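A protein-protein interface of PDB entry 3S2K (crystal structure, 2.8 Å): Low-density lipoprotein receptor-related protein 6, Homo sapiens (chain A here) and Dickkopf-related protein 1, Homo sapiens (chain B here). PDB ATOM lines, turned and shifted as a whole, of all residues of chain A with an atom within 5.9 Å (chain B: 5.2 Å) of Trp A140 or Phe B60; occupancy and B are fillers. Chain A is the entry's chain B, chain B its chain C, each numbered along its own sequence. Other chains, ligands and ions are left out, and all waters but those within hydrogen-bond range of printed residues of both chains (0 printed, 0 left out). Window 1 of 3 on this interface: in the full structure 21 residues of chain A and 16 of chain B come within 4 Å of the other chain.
Of the printed residues of chain B, Trp A140 touches Phe B60.
Gly A141 touches none of the printed residues of chain B.
Gly A142 touches none of the printed residues of chain B.
Of the printed residues of chain B, Met A250 touches Ile B59.
Of the printed residues of chain A, His B30 touches Glu A81.
Of the printed residues of chain A, Ile B59 touches Met A250 (3.9 Å).
Of chain A, only Glu A81 (3.9 Å), Trp A140 (3.6 Å), Arg A165 (2.6 Å) and Phe A209 (3.4 Å) come within 4 Å of Phe B60.
Printed residues of chain A within 4 Å of Arg B62: Arg A165 (3.4 Å).
The nearest printed residue of chain B that does not touch Trp A140 is His B30 (5.7 Å).
The nearest residue of chain A that does not touch Phe B60 is Arg A124 (4.1 Å).
The side-chain carboxylate of Glu A81 lies within hydrogen-bond range of a ring nitrogen (NE2) of His B30.
The guanidinium group (NH2) of Arg A165 lies within salt-bridge range of the side-chain carboxylate (OE2) of Glu B58 (3.1 Å).
NH1 of Arg A165 is in hydrogen-bond range of O of Phe B60, at 2.6 Å.
The guanidinium group (NE) of Arg A165 sits close to the guanidinium group (NH2) of Arg B62, 3.4 Å away.
Of the 21 printed residues of chain A, 5 touch a printed residue of chain B.
Hydrophobic or aromatic side chains of chain A that line the printed part of chain B: Trp A140, Phe A209 and Met A250.
Of the 9 printed residues of chain B, 6 touch a printed residue of chain A.
N of Trp A140 is in hydrogen-bond range of O of Ser A122, 2.7 Å away.
O of Arg A165 is in hydrogen-bond range of N of Leu A183, at 2.9 Å.
O of Phe A209 is in hydrogen-bond range of ND2 of Asn A167, at 2.9 Å.
NE of Arg B29 lies within hydrogen-bond range of O of Glu B58, 2.6 Å away.
The backbone NH (N) of Phe B31 sits at hydrogen-bond distance from the backbone carbonyl oxygen (O) of Ile B59 (2.8 Å).
The backbone NH (N) of Phe B60 is in hydrogen-bond range of the side-chain carboxylate (OE1) of Glu B58.
Among the printed residues, merely in contact across the chains: Glu A81 with Phe B31, Glu A81 with Phe B60, Trp A140 with Phe B60, Phe A209 with Phe B60 and Met A250 with Ile B59.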
ATOM      1  N   GLU A  81       8.347  25.048 -33.700  1.00  0.00           N
ATOM      2  CA  GLU A  81       6.902  24.850 -33.642  1.00  0.00           C
ATOM      3  C   GLU A  81       6.118  26.071 -34.114  1.00  0.00           C
ATOM      4  O   GLU A  81       4.981  25.946 -34.565  1.00  0.00           O
ATOM      5  CB  GLU A  81       6.464  24.443 -32.232  1.00  0.00           C
ATOM      6  CG  GLU A  81       7.143  23.179 -31.721  1.00  0.00           C
ATOM      7  CD  GLU A  81       6.499  22.626 -30.464  1.00  0.00           C
ATOM      8  OE1 GLU A  81       5.252  22.570 -30.405  1.00  0.00           O
ATOM      9  OE2 GLU A  81       7.240  22.244 -29.535  1.00  0.00           O
ATOM     10  N   ASP A 121      10.092  30.313 -22.127  1.00  0.00           N
ATOM     11  CA  ASP A 121       9.758  28.972 -21.673  1.00  0.00           C
ATOM     12  C   ASP A 121       8.813  28.300 -22.668  1.00  0.00           C
ATOM     13  O   ASP A 121       7.609  28.209 -22.434  1.00  0.00           O
ATOM     14  CB  ASP A 121       9.129  29.041 -20.279  1.00  0.00           C
ATOM     15  CG  ASP A 121       8.946  27.676 -19.641  1.00  0.00           C
ATOM     16  OD1 ASP A 121       9.493  26.681 -20.164  1.00  0.00           O
ATOM     17  OD2 ASP A 121       8.257  27.604 -18.600  1.00  0.00           O
ATOM     18  N   SER A 122       9.371  27.851 -23.789  1.00  0.00           N
ATOM     19  CA  SER A 122       8.613  27.151 -24.824  1.00  0.00           C
ATOM     20  C   SER A 122       7.595  28.036 -25.551  1.00  0.00           C
ATOM     21  O   SER A 122       6.392  27.918 -25.321  1.00  0.00           O
ATOM     22  CB  SER A 122       7.914  25.923 -24.237  1.00  0.00           C
ATOM     23  OG  SER A 122       8.851  25.012 -23.696  1.00  0.00           O
ATOM     24  N   PRO A 123       8.076  28.920 -26.439  1.00  0.00           N
ATOM     25  CA  PRO A 123       7.187  29.708 -27.298  1.00  0.00           C
ATOM     26  C   PRO A 123       6.602  28.805 -28.376  1.00  0.00           C
ATOM     27  O   PRO A 123       7.365  28.133 -29.073  1.00  0.00           O
ATOM     28  CB  PRO A 123       8.133  30.732 -27.941  1.00  0.00           C
ATOM     29  CG  PRO A 123       9.402  30.671 -27.138  1.00  0.00           C
ATOM     30  CD  PRO A 123       9.489  29.275 -26.639  1.00  0.00           C
ATOM     31  N   ARG A 124       5.279  28.785 -28.512  1.00  0.00           N
ATOM     32  CA  ARG A 124       4.623  27.863 -29.439  1.00  0.00           C
ATOM     33  C   ARG A 124       4.150  28.546 -30.718  1.00  0.00           C
ATOM     34  O   ARG A 124       4.850  28.534 -31.728  1.00  0.00           O
ATOM     35  CB  ARG A 124       3.458  27.137 -28.758  1.00  0.00           C
ATOM     36  CG  ARG A 124       2.676  26.193 -29.666  1.00  0.00           C
ATOM     37  CD  ARG A 124       3.600  25.232 -30.390  1.00  0.00           C
ATOM     38  NE  ARG A 124       2.891  24.113 -31.009  1.00  0.00           N
ATOM     39  CZ  ARG A 124       2.304  24.163 -32.199  1.00  0.00           C
ATOM     40  NH1 ARG A 124       2.327  25.286 -32.904  1.00  0.00           N
ATOM     41  NH2 ARG A 124       1.691  23.094 -32.686  1.00  0.00           N
ATOM     42  N   ALA A 125       2.961  29.135 -30.675  1.00  0.00           N
ATOM     43  CA  ALA A 125       2.376  29.749 -31.861  1.00  0.00           C
ATOM     44  C   ALA A 125       2.771  31.216 -31.976  1.00  0.00           C
ATOM     45  O   ALA A 125       3.065  31.870 -30.977  1.00  0.00           O
ATOM     46  CB  ALA A 125       0.865  29.596 -31.850  1.00  0.00           C
ATOM     47  N   THR A 138       2.126  32.492 -28.256  1.00  0.00           N
ATOM     48  CA  THR A 138       1.701  31.695 -27.112  1.00  0.00           C
ATOM     49  C   THR A 138       2.921  31.032 -26.485  1.00  0.00           C
ATOM     50  O   THR A 138       3.892  30.724 -27.176  1.00  0.00           O
ATOM     51  CB  THR A 138       0.689  30.610 -27.520  1.00  0.00           C
ATOM     52  OG1 THR A 138       1.345  29.607 -28.307  1.00  0.00           O
ATOM     53  CG2 THR A 138      -0.448  31.218 -28.322  1.00  0.00           C
ATOM     54  N   GLU A 139       2.870  30.815 -25.174  1.00  0.00           N
ATOM     55  CA  GLU A 139       3.994  30.231 -24.454  1.00  0.00           C
ATOM     56  C   GLU A 139       3.505  29.060 -23.602  1.00  0.00           C
ATOM     57  O   GLU A 139       2.488  29.167 -22.921  1.00  0.00           O
ATOM     58  CB  GLU A 139       4.669  31.301 -23.594  1.00  0.00           C
ATOM     59  CG  GLU A 139       6.124  31.029 -23.248  1.00  0.00           C
ATOM     60  CD  GLU A 139       6.855  32.285 -22.801  1.00  0.00           C
ATOM     61  OE1 GLU A 139       7.745  32.185 -21.929  1.00  0.00           O
ATOM     62  OE2 GLU A 139       6.538  33.371 -23.330  1.00  0.00           O
ATOM     63  N   TRP A 140       4.231  27.945 -23.657  1.00  0.00           N
ATOM     64  CA  TRP A 140       3.804  26.689 -23.038  1.00  0.00           C
ATOM     65  C   TRP A 140       4.753  26.224 -21.948  1.00  0.00           C
ATOM     66  O   TRP A 140       5.327  25.135 -22.046  1.00  0.00           O
ATOM     67  CB  TRP A 140       3.779  25.568 -24.076  1.00  0.00           C
ATOM     68  CG  TRP A 140       2.706  25.633 -25.104  1.00  0.00           C
ATOM     69  CD1 TRP A 140       1.941  26.709 -25.442  1.00  0.00           C
ATOM     70  CD2 TRP A 140       2.282  24.555 -25.942  1.00  0.00           C
ATOM     71  NE1 TRP A 140       1.063  26.364 -26.444  1.00  0.00           N
ATOM     72  CE2 TRP A 140       1.255  25.048 -26.768  1.00  0.00           C
ATOM     73  CE3 TRP A 140       2.674  23.221 -26.073  1.00  0.00           C
ATOM     74  CZ2 TRP A 140       0.612  24.249 -27.713  1.00  0.00           C
ATOM     75  CZ3 TRP A 140       2.036  22.429 -27.011  1.00  0.00           C
ATOM     76  CH2 TRP A 140       1.016  22.945 -27.819  1.00  0.00           C
ATOM     77  N   GLY A 141       4.931  27.021 -20.908  1.00  0.00           N
ATOM     78  CA  GLY A 141       5.855  26.629 -19.861  1.00  0.00           C
ATOM     79  C   GLY A 141       5.152  25.992 -18.684  1.00  0.00           C
ATOM     80  O   GLY A 141       4.158  25.284 -18.853  1.00  0.00           O
ATOM     81  N   GLY A 142       5.677  26.240 -17.489  1.00  0.00           N
ATOM     82  CA  GLY A 142       5.001  25.837 -16.273  1.00  0.00           C
ATOM     83  C   GLY A 142       3.792  26.726 -16.068  1.00  0.00           C
ATOM     84  O   GLY A 142       2.796  26.325 -15.463  1.00  0.00           O
ATOM     85  N   LYS A 143       3.884  27.944 -16.589  1.00  0.00           N
ATOM     86  CA  LYS A 143       2.813  28.920 -16.467  1.00  0.00           C
ATOM     87  C   LYS A 143       2.509  29.516 -17.834  1.00  0.00           C
ATOM     88  O   LYS A 143       2.921  30.633 -18.137  1.00  0.00           O
ATOM     89  CB  LYS A 143       3.206  30.024 -15.487  1.00  0.00           C
ATOM     90  CG  LYS A 143       2.073  30.963 -15.122  1.00  0.00           C
ATOM     91  CD  LYS A 143       2.511  31.967 -14.075  1.00  0.00           C
ATOM     92  CE  LYS A 143       1.362  32.858 -13.649  1.00  0.00           C
ATOM     93  NZ  LYS A 143       1.780  33.830 -12.601  1.00  0.00           N
ATOM     94  N   PRO A 144       1.787  28.758 -18.668  1.00  0.00           N
ATOM     95  CA  PRO A 144       1.484  29.183 -20.037  1.00  0.00           C
ATOM     96  C   PRO A 144       0.876  30.578 -20.069  1.00  0.00           C
ATOM     97  O   PRO A 144       0.225  30.988 -19.109  1.00  0.00           O
ATOM     98  CB  PRO A 144       0.463  28.143 -20.503  1.00  0.00           C
ATOM     99  CG  PRO A 144       0.778  26.936 -19.704  1.00  0.00           C
ATOM    100  CD  PRO A 144       1.207  27.441 -18.359  1.00  0.00           C
ATOM    101  N   LYS A 145       1.096  31.296 -21.166  1.00  0.00           N
ATOM    102  CA  LYS A 145       0.570  32.647 -21.320  1.00  0.00           C
ATOM    103  C   LYS A 145       0.614  33.064 -22.785  1.00  0.00           C
ATOM    104  O   LYS A 145       1.166  32.352 -23.624  1.00  0.00           O
ATOM    105  CB  LYS A 145       1.382  33.635 -20.479  1.00  0.00           C
ATOM    106  CG  LYS A 145       2.813  33.817 -20.959  1.00  0.00           C
ATOM    107  CD  LYS A 145       3.720  34.372 -19.867  1.00  0.00           C
ATOM    108  CE  LYS A 145       5.176  34.380 -20.320  1.00  0.00           C
ATOM    109  NZ  LYS A 145       6.090  34.981 -19.310  1.00  0.00           N
ATOM    110  N   GLY A 164      -4.142  27.940 -20.670  1.00  0.00           N
ATOM    111  CA  GLY A 164      -3.357  26.722 -20.787  1.00  0.00           C
ATOM    112  C   GLY A 164      -2.469  26.782 -22.015  1.00  0.00           C
ATOM    113  O   GLY A 164      -2.127  27.870 -22.473  1.00  0.00           O
ATOM    114  N   ARG A 165      -2.090  25.623 -22.550  1.00  0.00           N
ATOM    115  CA  ARG A 165      -1.319  25.574 -23.794  1.00  0.00           C
ATOM    116  C   ARG A 165      -2.151  26.078 -24.976  1.00  0.00           C
ATOM    117  O   ARG A 165      -2.995  25.355 -25.513  1.00  0.00           O
ATOM    118  CB  ARG A 165      -0.822  24.153 -24.069  1.00  0.00           C
ATOM    119  CG  ARG A 165       0.165  23.622 -23.036  1.00  0.00           C
ATOM    120  CD  ARG A 165       0.459  22.148 -23.248  1.00  0.00           C
ATOM    121  NE  ARG A 165      -0.701  21.310 -22.958  1.00  0.00           N
ATOM    122  CZ  ARG A 165      -0.733  19.992 -23.134  1.00  0.00           C
ATOM    123  NH1 ARG A 165       0.337  19.364 -23.604  1.00  0.00           N
ATOM    124  NH2 ARG A 165      -1.831  19.304 -22.845  1.00  0.00           N
ATOM    125  N   ALA A 166      -1.921  27.325 -25.373  1.00  0.00           N
ATOM    126  CA  ALA A 166      -2.673  27.922 -26.471  1.00  0.00           C
ATOM    127  C   ALA A 166      -2.000  27.635 -27.808  1.00  0.00           C
ATOM    128  O   ALA A 166      -0.772  27.539 -27.890  1.00  0.00           O
ATOM    129  CB  ALA A 166      -2.831  29.419 -26.259  1.00  0.00           C
ATOM    130  N   ASN A 167      -2.811  27.493 -28.852  1.00  0.00           N
ATOM    131  CA  ASN A 167      -2.304  27.152 -30.174  1.00  0.00           C
ATOM    132  C   ASN A 167      -3.093  27.869 -31.259  1.00  0.00           C
ATOM    133  O   ASN A 167      -4.099  28.513 -30.977  1.00  0.00           O
ATOM    134  CB  ASN A 167      -2.380  25.638 -30.393  1.00  0.00           C
ATOM    135  CG  ASN A 167      -1.508  25.170 -31.539  1.00  0.00           C
ATOM    136  OD1 ASN A 167      -0.343  25.548 -31.638  1.00  0.00           O
ATOM    137  ND2 ASN A 167      -2.073  24.347 -32.417  1.00  0.00           N
ATOM    138  N   LEU A 183      -5.327  23.713 -25.505  1.00  0.00           N
ATOM    139  CA  LEU A 183      -5.179  22.263 -25.485  1.00  0.00           C
ATOM    140  C   LEU A 183      -5.407  21.648 -24.103  1.00  0.00           C
ATOM    141  O   LEU A 183      -5.447  20.425 -23.965  1.00  0.00           O
ATOM    142  CB  LEU A 183      -3.808  21.860 -26.031  1.00  0.00           C
ATOM    143  CG  LEU A 183      -3.623  21.913 -27.550  1.00  0.00           C
ATOM    144  CD1 LEU A 183      -4.176  23.192 -28.153  1.00  0.00           C
ATOM    145  CD2 LEU A 183      -2.157  21.750 -27.904  1.00  0.00           C
ATOM    146  N   PHE A 209      -7.323  21.782 -32.061  1.00  0.00           N
ATOM    147  CA  PHE A 209      -5.884  21.973 -32.190  1.00  0.00           C
ATOM    148  C   PHE A 209      -5.517  23.170 -33.064  1.00  0.00           C
ATOM    149  O   PHE A 209      -5.014  24.177 -32.570  1.00  0.00           O
ATOM    150  CB  PHE A 209      -5.206  20.705 -32.713  1.00  0.00           C
ATOM    151  CG  PHE A 209      -3.711  20.763 -32.654  1.00  0.00           C
ATOM    152  CD1 PHE A 209      -3.058  20.721 -31.436  1.00  0.00           C
ATOM    153  CD2 PHE A 209      -2.959  20.872 -33.810  1.00  0.00           C
ATOM    154  CE1 PHE A 209      -1.681  20.783 -31.372  1.00  0.00           C
ATOM    155  CE2 PHE A 209      -1.579  20.934 -33.751  1.00  0.00           C
ATOM    156  CZ  PHE A 209      -0.940  20.890 -32.530  1.00  0.00           C
ATOM    157  N   MET A 250      -1.785  19.362 -38.465  1.00  0.00           N
ATOM    158  CA  MET A 250      -0.945  20.161 -37.587  1.00  0.00           C
ATOM    159  C   MET A 250      -1.353  21.634 -37.550  1.00  0.00           C
ATOM    160  O   MET A 250      -1.876  22.112 -36.543  1.00  0.00           O
ATOM    161  CB  MET A 250       0.532  19.995 -37.965  1.00  0.00           C
ATOM    162  CG  MET A 250       0.973  18.535 -38.020  1.00  0.00           C
ATOM    163  SD  MET A 250       0.264  17.548 -36.678  1.00  0.00           S
ATOM    164  CE  MET A 250       0.926  18.356 -35.227  1.00  0.00           C
ATOM    165  N   ARG B  29       6.745  12.106 -24.516  1.00  0.00           N
ATOM    166  CA  ARG B  29       6.760  12.222 -25.968  1.00  0.00           C
ATOM    167  C   ARG B  29       6.512  13.648 -26.443  1.00  0.00           C
ATOM    168  O   ARG B  29       5.679  14.368 -25.894  1.00  0.00           O
ATOM    169  CB  ARG B  29       5.805  11.228 -26.642  1.00  0.00           C
ATOM    170  CG  ARG B  29       4.356  11.314 -26.218  1.00  0.00           C
ATOM    171  CD  ARG B  29       3.530  10.254 -26.944  1.00  0.00           C
ATOM    172  NE  ARG B  29       2.145  10.213 -26.482  1.00  0.00           N
ATOM    173  CZ  ARG B  29       1.699   9.415 -25.516  1.00  0.00           C
ATOM    174  NH1 ARG B  29       2.530   8.584 -24.900  1.00  0.00           N
ATOM    175  NH2 ARG B  29       0.420   9.449 -25.165  1.00  0.00           N
ATOM    176  N   HIS B  30       7.281  14.050 -27.448  1.00  0.00           N
ATOM    177  CA  HIS B  30       7.106  15.333 -28.110  1.00  0.00           C
ATOM    178  C   HIS B  30       7.026  15.061 -29.602  1.00  0.00           C
ATOM    179  O   HIS B  30       8.008  14.651 -30.224  1.00  0.00           O
ATOM    180  CB  HIS B  30       8.268  16.277 -27.801  1.00  0.00           C
ATOM    181  CG  HIS B  30       7.953  17.720 -28.058  1.00  0.00           C
ATOM    182  ND1 HIS B  30       6.960  18.391 -27.382  1.00  0.00           N
ATOM    183  CD2 HIS B  30       8.497  18.610 -28.920  1.00  0.00           C
ATOM    184  CE1 HIS B  30       6.906  19.642 -27.815  1.00  0.00           C
ATOM    185  NE2 HIS B  30       7.826  19.800 -28.745  1.00  0.00           N
ATOM    186  N   PHE B  31       5.846  15.284 -30.166  1.00  0.00           N
ATOM    187  CA  PHE B  31       5.553  14.868 -31.531  1.00  0.00           C
ATOM    188  C   PHE B  31       5.631  13.348 -31.654  1.00  0.00           C
ATOM    189  O   PHE B  31       4.864  12.636 -31.005  1.00  0.00           O
ATOM    190  CB  PHE B  31       6.459  15.576 -32.543  1.00  0.00           C
ATOM    191  CG  PHE B  31       6.136  17.037 -32.730  1.00  0.00           C
ATOM    192  CD1 PHE B  31       5.063  17.430 -33.521  1.00  0.00           C
ATOM    193  CD2 PHE B  31       6.906  18.019 -32.120  1.00  0.00           C
ATOM    194  CE1 PHE B  31       4.764  18.773 -33.700  1.00  0.00           C
ATOM    195  CE2 PHE B  31       6.613  19.367 -32.295  1.00  0.00           C
ATOM    196  CZ  PHE B  31       5.541  19.741 -33.087  1.00  0.00           C
ATOM    197  N   LYS B  37      12.040  15.490 -20.426  1.00  0.00           N
ATOM    198  CA  LYS B  37      11.378  16.705 -19.966  1.00  0.00           C
ATOM    199  C   LYS B  37      11.427  16.772 -18.446  1.00  0.00           C
ATOM    200  O   LYS B  37      11.502  15.741 -17.777  1.00  0.00           O
ATOM    201  CB  LYS B  37       9.929  16.752 -20.464  1.00  0.00           C
ATOM    202  CG  LYS B  37       9.802  16.910 -21.975  1.00  0.00           C
ATOM    203  CD  LYS B  37       8.364  16.759 -22.440  1.00  0.00           C
ATOM    204  CE  LYS B  37       8.253  16.936 -23.947  1.00  0.00           C
ATOM    205  NZ  LYS B  37       6.852  16.790 -24.440  1.00  0.00           N
ATOM    206  N   GLU B  58      -2.375  12.330 -27.245  1.00  0.00           N
ATOM    207  CA  GLU B  58      -1.437  13.357 -26.806  1.00  0.00           C
ATOM    208  C   GLU B  58      -0.068  13.166 -27.448  1.00  0.00           C
ATOM    209  O   GLU B  58       0.533  12.097 -27.333  1.00  0.00           O
ATOM    210  CB  GLU B  58      -1.299  13.338 -25.281  1.00  0.00           C
ATOM    211  CG  GLU B  58      -0.465  14.473 -24.705  1.00  0.00           C
ATOM    212  CD  GLU B  58      -1.090  15.840 -24.941  1.00  0.00           C
ATOM    213  OE1 GLU B  58      -1.123  16.291 -26.107  1.00  0.00           O
ATOM    214  OE2 GLU B  58      -1.551  16.459 -23.958  1.00  0.00           O
ATOM    215  N   ILE B  59       0.415  14.202 -28.129  1.00  0.00           N
ATOM    216  CA  ILE B  59       1.771  14.199 -28.678  1.00  0.00           C
ATOM    217  C   ILE B  59       2.632  15.247 -27.980  1.00  0.00           C
ATOM    218  O   ILE B  59       3.843  15.311 -28.189  1.00  0.00           O
ATOM    219  CB  ILE B  59       1.794  14.458 -30.200  1.00  0.00           C
ATOM    220  CG1 ILE B  59       1.311  15.874 -30.511  1.00  0.00           C
ATOM    221  CG2 ILE B  59       0.952  13.428 -30.935  1.00  0.00           C
ATOM    222  CD1 ILE B  59       1.541  16.286 -31.947  1.00  0.00           C
ATOM    223  N   PHE B  60       1.994  16.081 -27.162  1.00  0.00           N
ATOM    224  CA  PHE B  60       2.716  17.033 -26.327  1.00  0.00           C
ATOM    225  C   PHE B  60       2.511  16.663 -24.867  1.00  0.00           C
ATOM    226  O   PHE B  60       1.672  17.234 -24.176  1.00  0.00           O
ATOM    227  CB  PHE B  60       2.259  18.466 -26.604  1.00  0.00           C
ATOM    228  CG  PHE B  60       2.328  18.849 -28.054  1.00  0.00           C
ATOM    229  CD1 PHE B  60       3.519  18.738 -28.758  1.00  0.00           C
ATOM    230  CD2 PHE B  60       1.203  19.313 -28.717  1.00  0.00           C
ATOM    231  CE1 PHE B  60       3.584  19.081 -30.099  1.00  0.00           C
ATOM    232  CE2 PHE B  60       1.262  19.659 -30.054  1.00  0.00           C
ATOM    233  CZ  PHE B  60       2.452  19.543 -30.747  1.00  0.00           C
ATOM    234  N   GLN B  61       3.293  15.691 -24.414  1.00  0.00           N
ATOM    235  CA  GLN B  61       3.136  15.099 -23.093  1.00  0.00           C
ATOM    236  C   GLN B  61       3.945  15.845 -22.035  1.00  0.00           C
ATOM    237  O   GLN B  61       5.140  16.082 -22.212  1.00  0.00           O
ATOM    238  CB  GLN B  61       3.561  13.628 -23.149  1.00  0.00           C
ATOM    239  CG  GLN B  61       3.406  12.855 -21.856  1.00  0.00           C
ATOM    240  CD  GLN B  61       3.826  11.404 -22.001  1.00  0.00           C
ATOM    241  OE1 GLN B  61       4.076  10.930 -23.109  1.00  0.00           O
ATOM    242  NE2 GLN B  61       3.910  10.694 -20.881  1.00  0.00           N
ATOM    243  N   ARG B  62       3.285  16.226 -20.945  1.00  0.00           N
ATOM    244  CA  ARG B  62       3.973  16.782 -19.784  1.00  0.00           C
ATOM    245  C   ARG B  62       4.452  15.649 -18.890  1.00  0.00           C
ATOM    246  O   ARG B  62       3.978  14.519 -19.002  1.00  0.00           O
ATOM    247  CB  ARG B  62       3.038  17.667 -18.960  1.00  0.00           C
ATOM    248  CG  ARG B  62       2.645  18.984 -19.580  1.00  0.00           C
ATOM    249  CD  ARG B  62       1.942  19.843 -18.539  1.00  0.00           C
ATOM    250  NE  ARG B  62       1.492  21.125 -19.069  1.00  0.00           N
ATOM    251  CZ  ARG B  62       0.227  21.404 -19.369  1.00  0.00           C
ATOM    252  NH1 ARG B  62      -0.718  20.491 -19.188  1.00  0.00           N
ATOM    253  NH2 ARG B  62      -0.094  22.599 -19.845  1.00  0.00           N
